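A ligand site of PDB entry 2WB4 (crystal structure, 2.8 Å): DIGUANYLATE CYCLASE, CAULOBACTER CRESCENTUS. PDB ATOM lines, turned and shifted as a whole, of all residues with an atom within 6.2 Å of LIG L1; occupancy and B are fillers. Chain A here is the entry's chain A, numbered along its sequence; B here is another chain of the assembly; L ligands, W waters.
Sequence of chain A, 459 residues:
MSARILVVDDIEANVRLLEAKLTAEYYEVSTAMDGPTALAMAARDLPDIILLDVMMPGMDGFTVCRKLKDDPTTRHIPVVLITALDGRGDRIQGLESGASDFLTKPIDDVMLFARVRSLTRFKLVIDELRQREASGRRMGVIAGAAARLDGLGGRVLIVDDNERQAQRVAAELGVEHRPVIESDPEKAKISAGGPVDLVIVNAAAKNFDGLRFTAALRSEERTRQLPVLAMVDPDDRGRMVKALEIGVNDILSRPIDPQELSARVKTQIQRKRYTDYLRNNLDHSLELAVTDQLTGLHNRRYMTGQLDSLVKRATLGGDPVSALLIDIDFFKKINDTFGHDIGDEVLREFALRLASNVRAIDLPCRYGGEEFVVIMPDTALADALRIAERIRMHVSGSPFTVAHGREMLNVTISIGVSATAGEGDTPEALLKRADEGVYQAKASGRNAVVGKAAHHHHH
The side-chain carboxylate (OD1) of Asp 383 lies within salt-bridge range of the guanidinium group (NE) of Arg 386, 3.7 Å away.
The side-chain hydroxyl (OG1) of Thr 379 sits at hydrogen-bond distance from the backbone carbonyl oxygen (O) of Pro 377 (2.8 Å).
The side-chain carboxylate (OD2) of Asp 362 is in hydrogen-bond range of the backbone NH (N) of Arg 359 (3.0 Å).
The guanidinium group (NH2) of Arg 390 lies within hydrogen-bond range of the backbone carbonyl oxygen (O) of Asn 357, at 3.0 Å.
An oxygen (O11) of LIG L1 sits close to the side-chain carboxylate (OD1) of Asp 383, at 3.4 Å.
CA of Val 358 touches O14 of LIG L1, 3.9 Å away.
Thr 379 touches LIG L1.
CG1 of Ile 387 touches N7 of LIG L1 (3.5 Å).
Hydrophobic or aromatic side chains within 4 Å of LIG L1: Ile 387.
The nearest printed residue that does not touch LIG L1 is Ile 361 (4.1 Å).
O1 of LIG L1 is in salt-bridge range of NH2 of Arg 359 (2.9 Å).
NH2 of Arg 313 of chain B is in salt-bridge range of O8 of LG2 L2 (2.9 Å).
N4 of LG2 L2 lies within hydrogen-bond range of O of Arg 313 of chain B, 2.9 Å away.
The side-chain carboxylate of Asp 362 lies within hydrogen-bond range of a nitrogen (N8) of LIG L1.
An oxygen (O9) of LIG L1 lies within salt-bridge range of the guanidinium group of Arg 386 (3.9 Å).
O11 of LG2 L2 sits at hydrogen-bond distance from N of Val 358 (3.3 Å).
A nitrogen (N7) of LG2 L2 lies within hydrogen-bond range of the guanidinium group of Arg 359, 2.9 Å away.
NH2 of Arg 313 of chain B is in hydrogen-bond range of O7 of LIG L1 (2.7 Å).
An oxygen (O14) of LIG L1 lies within hydrogen-bond range of the guanidinium group (NH2) of Arg 390 (2.9 Å).
O14 of LIG L1 lies within hydrogen-bond range of N of Arg 359 (3.4 Å).
A nitrogen (N10) of LG2 L2 sits close to the guanidinium group of Arg 390 (3.4 Å).
O8 of LIG L1 is in hydrogen-bond range of N8 of LG2 L2, 2.7 Å away.
Water W2 lies within hydrogen-bond range of O1 of LIG L1 (2.6 Å) and NH1 of Arg 313 of chain B (3.4 Å).
Water W3 lies within hydrogen-bond range of O8 of LIG L1 (2.7 Å) and NH1 of Arg 390 (2.9 Å).
Water W1 bridges a nitrogen (N10) of LIG L1 (2.8 Å) and the side-chain hydroxyl of Thr 379 (3.4 Å).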
ATOM      1  N   ASN A 357      -2.739  35.633 -11.712  1.00  0.00           N
ATOM      2  CA  ASN A 357      -3.678  34.506 -11.738  1.00  0.00           C
ATOM      3  C   ASN A 357      -3.341  33.359 -12.667  1.00  0.00           C
ATOM      4  O   ASN A 357      -4.221  32.616 -13.084  1.00  0.00           O
ATOM      5  CB  ASN A 357      -5.059  35.035 -12.024  1.00  0.00           C
ATOM      6  CG  ASN A 357      -5.657  35.682 -10.821  1.00  0.00           C
ATOM      7  OD1 ASN A 357      -6.001  35.007  -9.856  1.00  0.00           O
ATOM      8  ND2 ASN A 357      -5.731  37.010 -10.827  1.00  0.00           N
ATOM      9  N   VAL A 358      -2.053  33.184 -12.912  1.00  0.00           N
ATOM     10  CA  VAL A 358      -1.546  32.316 -13.943  1.00  0.00           C
ATOM     11  C   VAL A 358      -0.190  31.898 -13.436  1.00  0.00           C
ATOM     12  O   VAL A 358       0.454  32.671 -12.761  1.00  0.00           O
ATOM     13  CB  VAL A 358      -1.444  33.146 -15.280  1.00  0.00           C
ATOM     14  CG1 VAL A 358      -0.204  32.785 -16.070  1.00  0.00           C
ATOM     15  CG2 VAL A 358      -2.700  32.973 -16.091  1.00  0.00           C
ATOM     16  N   ARG A 359       0.241  30.681 -13.745  1.00  0.00           N
ATOM     17  CA  ARG A 359       1.487  30.175 -13.203  1.00  0.00           C
ATOM     18  C   ARG A 359       2.653  30.871 -13.822  1.00  0.00           C
ATOM     19  O   ARG A 359       2.516  31.459 -14.881  1.00  0.00           O
ATOM     20  CB  ARG A 359       1.642  28.677 -13.415  1.00  0.00           C
ATOM     21  CG  ARG A 359       0.558  27.849 -12.764  1.00  0.00           C
ATOM     22  CD  ARG A 359       0.681  26.393 -13.095  1.00  0.00           C
ATOM     23  NE  ARG A 359      -0.491  25.661 -12.624  1.00  0.00           N
ATOM     24  CZ  ARG A 359      -0.580  24.337 -12.518  1.00  0.00           C
ATOM     25  NH1 ARG A 359       0.442  23.590 -12.847  1.00  0.00           N
ATOM     26  NH2 ARG A 359      -1.694  23.777 -12.079  1.00  0.00           N
ATOM     27  N   ILE A 361       5.385  29.719 -15.057  1.00  0.00           N
ATOM     28  CA  ILE A 361       5.863  29.080 -16.280  1.00  0.00           C
ATOM     29  C   ILE A 361       5.076  29.506 -17.501  1.00  0.00           C
ATOM     30  O   ILE A 361       5.527  29.324 -18.605  1.00  0.00           O
ATOM     31  CB  ILE A 361       5.809  27.538 -16.212  1.00  0.00           C
ATOM     32  CG1 ILE A 361       6.889  26.920 -17.112  1.00  0.00           C
ATOM     33  CG2 ILE A 361       4.410  27.014 -16.622  1.00  0.00           C
ATOM     34  CD1 ILE A 361       8.294  27.531 -16.949  1.00  0.00           C
ATOM     35  N   ASP A 362       3.903  30.066 -17.298  1.00  0.00           N
ATOM     36  CA  ASP A 362       3.137  30.660 -18.378  1.00  0.00           C
ATOM     37  C   ASP A 362       3.815  31.949 -18.803  1.00  0.00           C
ATOM     38  O   ASP A 362       4.702  32.450 -18.122  1.00  0.00           O
ATOM     39  CB  ASP A 362       1.689  30.911 -17.947  1.00  0.00           C
ATOM     40  CG  ASP A 362       0.941  29.602 -17.519  1.00  0.00           C
ATOM     41  OD1 ASP A 362       1.172  28.490 -18.089  1.00  0.00           O
ATOM     42  OD2 ASP A 362       0.096  29.708 -16.580  1.00  0.00           O
ATOM     43  N   MET A 376       0.826  29.003 -22.739  1.00  0.00           N
ATOM     44  CA  MET A 376       0.831  27.987 -21.695  1.00  0.00           C
ATOM     45  C   MET A 376       1.528  26.750 -22.166  1.00  0.00           C
ATOM     46  O   MET A 376       0.917  25.928 -22.783  1.00  0.00           O
ATOM     47  CB  MET A 376      -0.589  27.669 -21.304  1.00  0.00           C
ATOM     48  CG  MET A 376      -1.252  28.824 -20.695  1.00  0.00           C
ATOM     49  SD  MET A 376      -3.040  28.843 -20.852  1.00  0.00           S
ATOM     50  CE  MET A 376      -3.257  29.163 -22.597  1.00  0.00           C
ATOM     51  N   PRO A 377       2.795  26.598 -21.859  1.00  0.00           N
ATOM     52  CA  PRO A 377       3.435  25.368 -22.226  1.00  0.00           C
ATOM     53  C   PRO A 377       2.802  24.172 -21.547  1.00  0.00           C
ATOM     54  O   PRO A 377       2.172  24.303 -20.510  1.00  0.00           O
ATOM     55  CB  PRO A 377       4.873  25.528 -21.706  1.00  0.00           C
ATOM     56  CG  PRO A 377       4.980  26.887 -21.185  1.00  0.00           C
ATOM     57  CD  PRO A 377       3.629  27.392 -20.943  1.00  0.00           C
ATOM     58  N   ASP A 378       3.007  23.013 -22.152  1.00  0.00           N
ATOM     59  CA  ASP A 378       2.543  21.706 -21.650  1.00  0.00           C
ATOM     60  C   ASP A 378       1.077  21.709 -21.216  1.00  0.00           C
ATOM     61  O   ASP A 378       0.739  21.181 -20.191  1.00  0.00           O
ATOM     62  CB  ASP A 378       3.480  21.166 -20.556  1.00  0.00           C
ATOM     63  CG  ASP A 378       3.520  19.622 -20.495  1.00  0.00           C
ATOM     64  OD1 ASP A 378       2.959  18.976 -21.425  1.00  0.00           O
ATOM     65  OD2 ASP A 378       4.126  19.046 -19.535  1.00  0.00           O
ATOM     66  N   THR A 379       0.233  22.289 -22.057  1.00  0.00           N
ATOM     67  CA  THR A 379      -1.190  22.478 -21.773  1.00  0.00           C
ATOM     68  C   THR A 379      -2.053  22.202 -23.010  1.00  0.00           C
ATOM     69  O   THR A 379      -1.854  22.794 -24.061  1.00  0.00           O
ATOM     70  CB  THR A 379      -1.428  23.896 -21.234  1.00  0.00           C
ATOM     71  OG1 THR A 379      -0.547  24.090 -20.131  1.00  0.00           O
ATOM     72  CG2 THR A 379      -2.844  24.075 -20.719  1.00  0.00           C
ATOM     73  N   ASP A 383      -7.692  22.111 -20.409  1.00  0.00           N
ATOM     74  CA  ASP A 383      -7.077  22.921 -19.363  1.00  0.00           C
ATOM     75  C   ASP A 383      -6.937  24.400 -19.715  1.00  0.00           C
ATOM     76  O   ASP A 383      -7.035  25.258 -18.849  1.00  0.00           O
ATOM     77  CB  ASP A 383      -5.701  22.376 -19.022  1.00  0.00           C
ATOM     78  CG  ASP A 383      -5.745  21.028 -18.282  1.00  0.00           C
ATOM     79  OD1 ASP A 383      -6.768  20.702 -17.623  1.00  0.00           O
ATOM     80  OD2 ASP A 383      -4.734  20.276 -18.352  1.00  0.00           O
ATOM     81  N   ARG A 386     -10.262  26.115 -19.196  1.00  0.00           N
ATOM     82  CA  ARG A 386     -10.522  26.232 -17.789  1.00  0.00           C
ATOM     83  C   ARG A 386      -9.743  27.382 -17.192  1.00  0.00           C
ATOM     84  O   ARG A 386     -10.271  28.186 -16.450  1.00  0.00           O
ATOM     85  CB  ARG A 386     -10.111  24.934 -17.128  1.00  0.00           C
ATOM     86  CG  ARG A 386     -10.969  24.530 -16.001  1.00  0.00           C
ATOM     87  CD  ARG A 386     -11.025  23.026 -15.839  1.00  0.00           C
ATOM     88  NE  ARG A 386      -9.977  22.284 -16.549  1.00  0.00           N
ATOM     89  CZ  ARG A 386     -10.164  21.125 -17.180  1.00  0.00           C
ATOM     90  NH1 ARG A 386     -11.363  20.534 -17.234  1.00  0.00           N
ATOM     91  NH2 ARG A 386      -9.149  20.544 -17.756  1.00  0.00           N
ATOM     92  N   ILE A 387      -8.482  27.469 -17.552  1.00  0.00           N
ATOM     93  CA  ILE A 387      -7.670  28.642 -17.235  1.00  0.00           C
ATOM     94  C   ILE A 387      -8.301  29.932 -17.741  1.00  0.00           C
ATOM     95  O   ILE A 387      -8.300  30.926 -17.036  1.00  0.00           O
ATOM     96  CB  ILE A 387      -6.326  28.538 -17.871  1.00  0.00           C
ATOM     97  CG1 ILE A 387      -5.567  27.359 -17.278  1.00  0.00           C
ATOM     98  CG2 ILE A 387      -5.570  29.826 -17.661  1.00  0.00           C
ATOM     99  CD1 ILE A 387      -4.333  26.965 -18.051  1.00  0.00           C
ATOM    100  N   ARG A 390     -11.404  30.936 -15.770  1.00  0.00           N
ATOM    101  CA  ARG A 390     -10.943  31.463 -14.516  1.00  0.00           C
ATOM    102  C   ARG A 390     -10.569  32.947 -14.678  1.00  0.00           C
ATOM    103  O   ARG A 390     -11.098  33.812 -13.982  1.00  0.00           O
ATOM    104  CB  ARG A 390      -9.776  30.623 -14.034  1.00  0.00           C
ATOM    105  CG  ARG A 390      -9.234  30.936 -12.667  1.00  0.00           C
ATOM    106  CD  ARG A 390      -8.227  29.855 -12.257  1.00  0.00           C
ATOM    107  NE  ARG A 390      -6.859  30.161 -12.683  1.00  0.00           N
ATOM    108  CZ  ARG A 390      -5.987  29.274 -13.178  1.00  0.00           C
ATOM    109  NH1 ARG A 390      -6.330  28.015 -13.395  1.00  0.00           N
ATOM    110  NH2 ARG A 390      -4.767  29.662 -13.521  1.00  0.00           N
ATOM    111  N   ARG B 313       5.866  25.677  -6.068  1.00  0.00           N
ATOM    112  CA  ARG B 313       5.002  24.699  -6.708  1.00  0.00           C
ATOM    113  C   ARG B 313       5.593  23.306  -6.651  1.00  0.00           C
ATOM    114  O   ARG B 313       4.853  22.332  -6.620  1.00  0.00           O
ATOM    115  CB  ARG B 313       4.743  25.061  -8.147  1.00  0.00           C
ATOM    116  CG  ARG B 313       3.939  24.020  -8.919  1.00  0.00           C
ATOM    117  CD  ARG B 313       3.328  24.540 -10.198  1.00  0.00           C
ATOM    118  NE  ARG B 313       2.351  25.576  -9.898  1.00  0.00           N
ATOM    119  CZ  ARG B 313       1.112  25.344  -9.480  1.00  0.00           C
ATOM    120  NH1 ARG B 313       0.672  24.100  -9.331  1.00  0.00           N
ATOM    121  NH2 ARG B 313       0.307  26.360  -9.223  1.00  0.00           N
HETATM  122  P1  LIG L   1      -2.794  19.987 -11.908  1.00  0.00           P
HETATM  123  O1  LIG L   1      -1.608  20.913 -11.913  1.00  0.00           O
HETATM  124  O2  LIG L   1      -2.610  18.531 -11.472  1.00  0.00           O
HETATM  125  O3  LIG L   1      -3.831  20.600 -10.835  1.00  0.00           O
HETATM  126  C1  LIG L   1      -4.915  19.852 -10.306  1.00  0.00           C
HETATM  127  C2  LIG L   1      -5.850  20.748  -9.480  1.00  0.00           C
HETATM  128  O4  LIG L   1      -5.158  21.148  -8.308  1.00  0.00           O
HETATM  129  C3  LIG L   1      -6.363  22.011 -10.160  1.00  0.00           C
HETATM  130  O5  LIG L   1      -7.559  21.753 -10.921  1.00  0.00           O
HETATM  131  C4  LIG L   1      -6.629  22.866  -8.924  1.00  0.00           C
HETATM  132  O6  LIG L   1      -7.933  22.624  -8.378  1.00  0.00           O
HETATM  133  C5  LIG L   1      -5.538  22.475  -7.924  1.00  0.00           C
HETATM  134  N1  LIG L   1      -4.370  23.412  -7.966  1.00  0.00           N
HETATM  135  C6  LIG L   1      -3.098  23.103  -8.368  1.00  0.00           C
HETATM  136  N2  LIG L   1      -2.326  24.222  -8.262  1.00  0.00           N
HETATM  137  C7  LIG L   1      -3.105  25.224  -7.801  1.00  0.00           C
HETATM  138  C8  LIG L   1      -2.875  26.574  -7.507  1.00  0.00           C
HETATM  139  O7  LIG L   1      -1.782  27.171  -7.637  1.00  0.00           O
HETATM  140  N3  LIG L   1      -3.861  27.316  -7.058  1.00  0.00           N
HETATM  141  C9  LIG L   1      -5.072  26.825  -6.877  1.00  0.00           C
HETATM  142  N4  LIG L   1      -5.995  27.699  -6.418  1.00  0.00           N
HETATM  143  N5  LIG L   1      -5.366  25.531  -7.162  1.00  0.00           N
HETATM  144  C10 LIG L   1      -4.392  24.718  -7.627  1.00  0.00           C
HETATM  145  P2  LIG L   1      -7.708  22.811 -12.111  1.00  0.00           P
HETATM  146  O8  LIG L   1      -7.440  24.194 -11.570  1.00  0.00           O
HETATM  147  O9  LIG L   1      -9.062  22.645 -12.772  1.00  0.00           O
HETATM  148  O10 LIG L   1      -6.554  22.520 -13.188  1.00  0.00           O
HETATM  149  C11 LIG L   1      -6.257  21.210 -13.599  1.00  0.00           C
HETATM  150  C12 LIG L   1      -5.082  21.298 -14.533  1.00  0.00           C
HETATM  151  O11 LIG L   1      -5.077  22.476 -15.332  1.00  0.00           O
HETATM  152  C13 LIG L   1      -3.809  21.322 -13.736  1.00  0.00           C
HETATM  153  O12 LIG L   1      -3.467  20.002 -13.360  1.00  0.00           O
HETATM  154  C14 LIG L   1      -2.830  21.969 -14.714  1.00  0.00           C
HETATM  155  O13 LIG L   1      -2.249  21.015 -15.579  1.00  0.00           O
HETATM  156  C15 LIG L   1      -3.708  22.910 -15.529  1.00  0.00           C
HETATM  157  N6  LIG L   1      -3.600  24.335 -15.126  1.00  0.00           N
HETATM  158  C16 LIG L   1      -4.519  25.033 -14.429  1.00  0.00           C
HETATM  159  N7  LIG L   1      -4.127  26.309 -14.281  1.00  0.00           N
HETATM  160  C17 LIG L   1      -2.941  26.394 -14.901  1.00  0.00           C
HETATM  161  C18 LIG L   1      -2.061  27.443 -15.084  1.00  0.00           C
HETATM  162  O14 LIG L   1      -2.299  28.575 -14.644  1.00  0.00           O
HETATM  163  N8  LIG L   1      -0.943  27.214 -15.746  1.00  0.00           N
HETATM  164  C19 LIG L   1      -0.662  26.012 -16.246  1.00  0.00           C
HETATM  165  N9  LIG L   1       0.472  25.846 -16.920  1.00  0.00           N
HETATM  166  N10 LIG L   1      -1.468  24.963 -16.083  1.00  0.00           N
HETATM  167  C20 LIG L   1      -2.616  25.153 -15.427  1.00  0.00           C
HETATM  168  P1  LG2 L   2      -2.564  30.713  -5.325  1.00  0.00           P
HETATM  169  O1  LG2 L   2      -3.758  29.801  -5.500  1.00  0.00           O
HETATM  170  O2  LG2 L   2      -2.535  31.578  -4.109  1.00  0.00           O
HETATM  171  O3  LG2 L   2      -1.223  29.841  -5.121  1.00  0.00           O
HETATM  172  C1  LG2 L   2      -0.048  30.547  -4.797  1.00  0.00           C
HETATM  173  C2  LG2 L   2       1.184  29.745  -5.206  1.00  0.00           C
HETATM  174  O4  LG2 L   2       1.284  28.612  -4.370  1.00  0.00           O
HETATM  175  C3  LG2 L   2       1.252  29.235  -6.644  1.00  0.00           C
HETATM  176  O5  LG2 L   2       2.118  30.108  -7.369  1.00  0.00           O
HETATM  177  C4  LG2 L   2       1.864  27.860  -6.484  1.00  0.00           C
HETATM  178  O6  LG2 L   2       3.285  27.998  -6.563  1.00  0.00           O
HETATM  179  C5  LG2 L   2       1.542  27.409  -5.080  1.00  0.00           C
HETATM  180  N1  LG2 L   2       0.358  26.514  -5.009  1.00  0.00           N
HETATM  181  C6  LG2 L   2      -0.891  26.853  -4.641  1.00  0.00           C
HETATM  182  N2  LG2 L   2      -1.699  25.756  -4.706  1.00  0.00           N
HETATM  183  C7  LG2 L   2      -0.926  24.738  -5.113  1.00  0.00           C
HETATM  184  C8  LG2 L   2      -1.207  23.411  -5.357  1.00  0.00           C
HETATM  185  O7  LG2 L   2      -2.356  22.969  -5.198  1.00  0.00           O
HETATM  186  N3  LG2 L   2      -0.212  22.612  -5.771  1.00  0.00           N
HETATM  187  C9  LG2 L   2       1.030  23.088  -5.965  1.00  0.00           C
HETATM  188  N4  LG2 L   2       1.988  22.241  -6.383  1.00  0.00           N
HETATM  189  N5  LG2 L   2       1.331  24.396  -5.744  1.00  0.00           N
HETATM  190  C10 LG2 L   2       0.359  25.218  -5.301  1.00  0.00           C
HETATM  191  P2  LG2 L   2       1.875  29.971  -8.919  1.00  0.00           P
HETATM  192  O8  LG2 L   2       2.236  28.580  -9.322  1.00  0.00           O
HETATM  193  O9  LG2 L   2       2.579  31.119  -9.608  1.00  0.00           O
HETATM  194  O10 LG2 L   2       0.347  30.276  -9.269  1.00  0.00           O
HETATM  195  C11 LG2 L   2      -0.109  31.562  -8.877  1.00  0.00           C
HETATM  196  C12 LG2 L   2      -1.619  31.695  -8.946  1.00  0.00           C
HETATM  197  O11 LG2 L   2      -2.106  31.227 -10.218  1.00  0.00           O
HETATM  198  C13 LG2 L   2      -2.334  30.916  -7.847  1.00  0.00           C
HETATM  199  O12 LG2 L   2      -2.402  31.692  -6.636  1.00  0.00           O
HETATM  200  C14 LG2 L   2      -3.661  30.736  -8.543  1.00  0.00           C
HETATM  201  O13 LG2 L   2      -4.412  31.928  -8.297  1.00  0.00           O
HETATM  202  C15 LG2 L   2      -3.369  30.569 -10.047  1.00  0.00           C
HETATM  203  N6  LG2 L   2      -3.251  29.126 -10.413  1.00  0.00           N
HETATM  204  C16 LG2 L   2      -2.129  28.469 -10.819  1.00  0.00           C
HETATM  205  N7  LG2 L   2      -2.445  27.162 -11.032  1.00  0.00           N
HETATM  206  C17 LG2 L   2      -3.770  27.028 -10.753  1.00  0.00           C
HETATM  207  C18 LG2 L   2      -4.657  25.962 -10.785  1.00  0.00           C
HETATM  208  O14 LG2 L   2      -4.308  24.824 -11.134  1.00  0.00           O
HETATM  209  N8  LG2 L   2      -5.917  26.120 -10.470  1.00  0.00           N
HETATM  210  C19 LG2 L   2      -6.367  27.319 -10.108  1.00  0.00           C
HETATM  211  N9  LG2 L   2      -7.672  27.423  -9.788  1.00  0.00           N
HETATM  212  N10 LG2 L   2      -5.548  28.405 -10.060  1.00  0.00           N
HETATM  213  C20 LG2 L   2      -4.260  28.262 -10.385  1.00  0.00           C
HETATM  214  O   HOH W   1      -0.055  22.779 -17.017  1.00  0.00           O
HETATM  215  O   HOH W   2      -0.068  20.841  -9.852  1.00  0.00           O
HETATM  216  O   HOH W   3      -8.490  26.160 -13.072  1.00  0.00           O
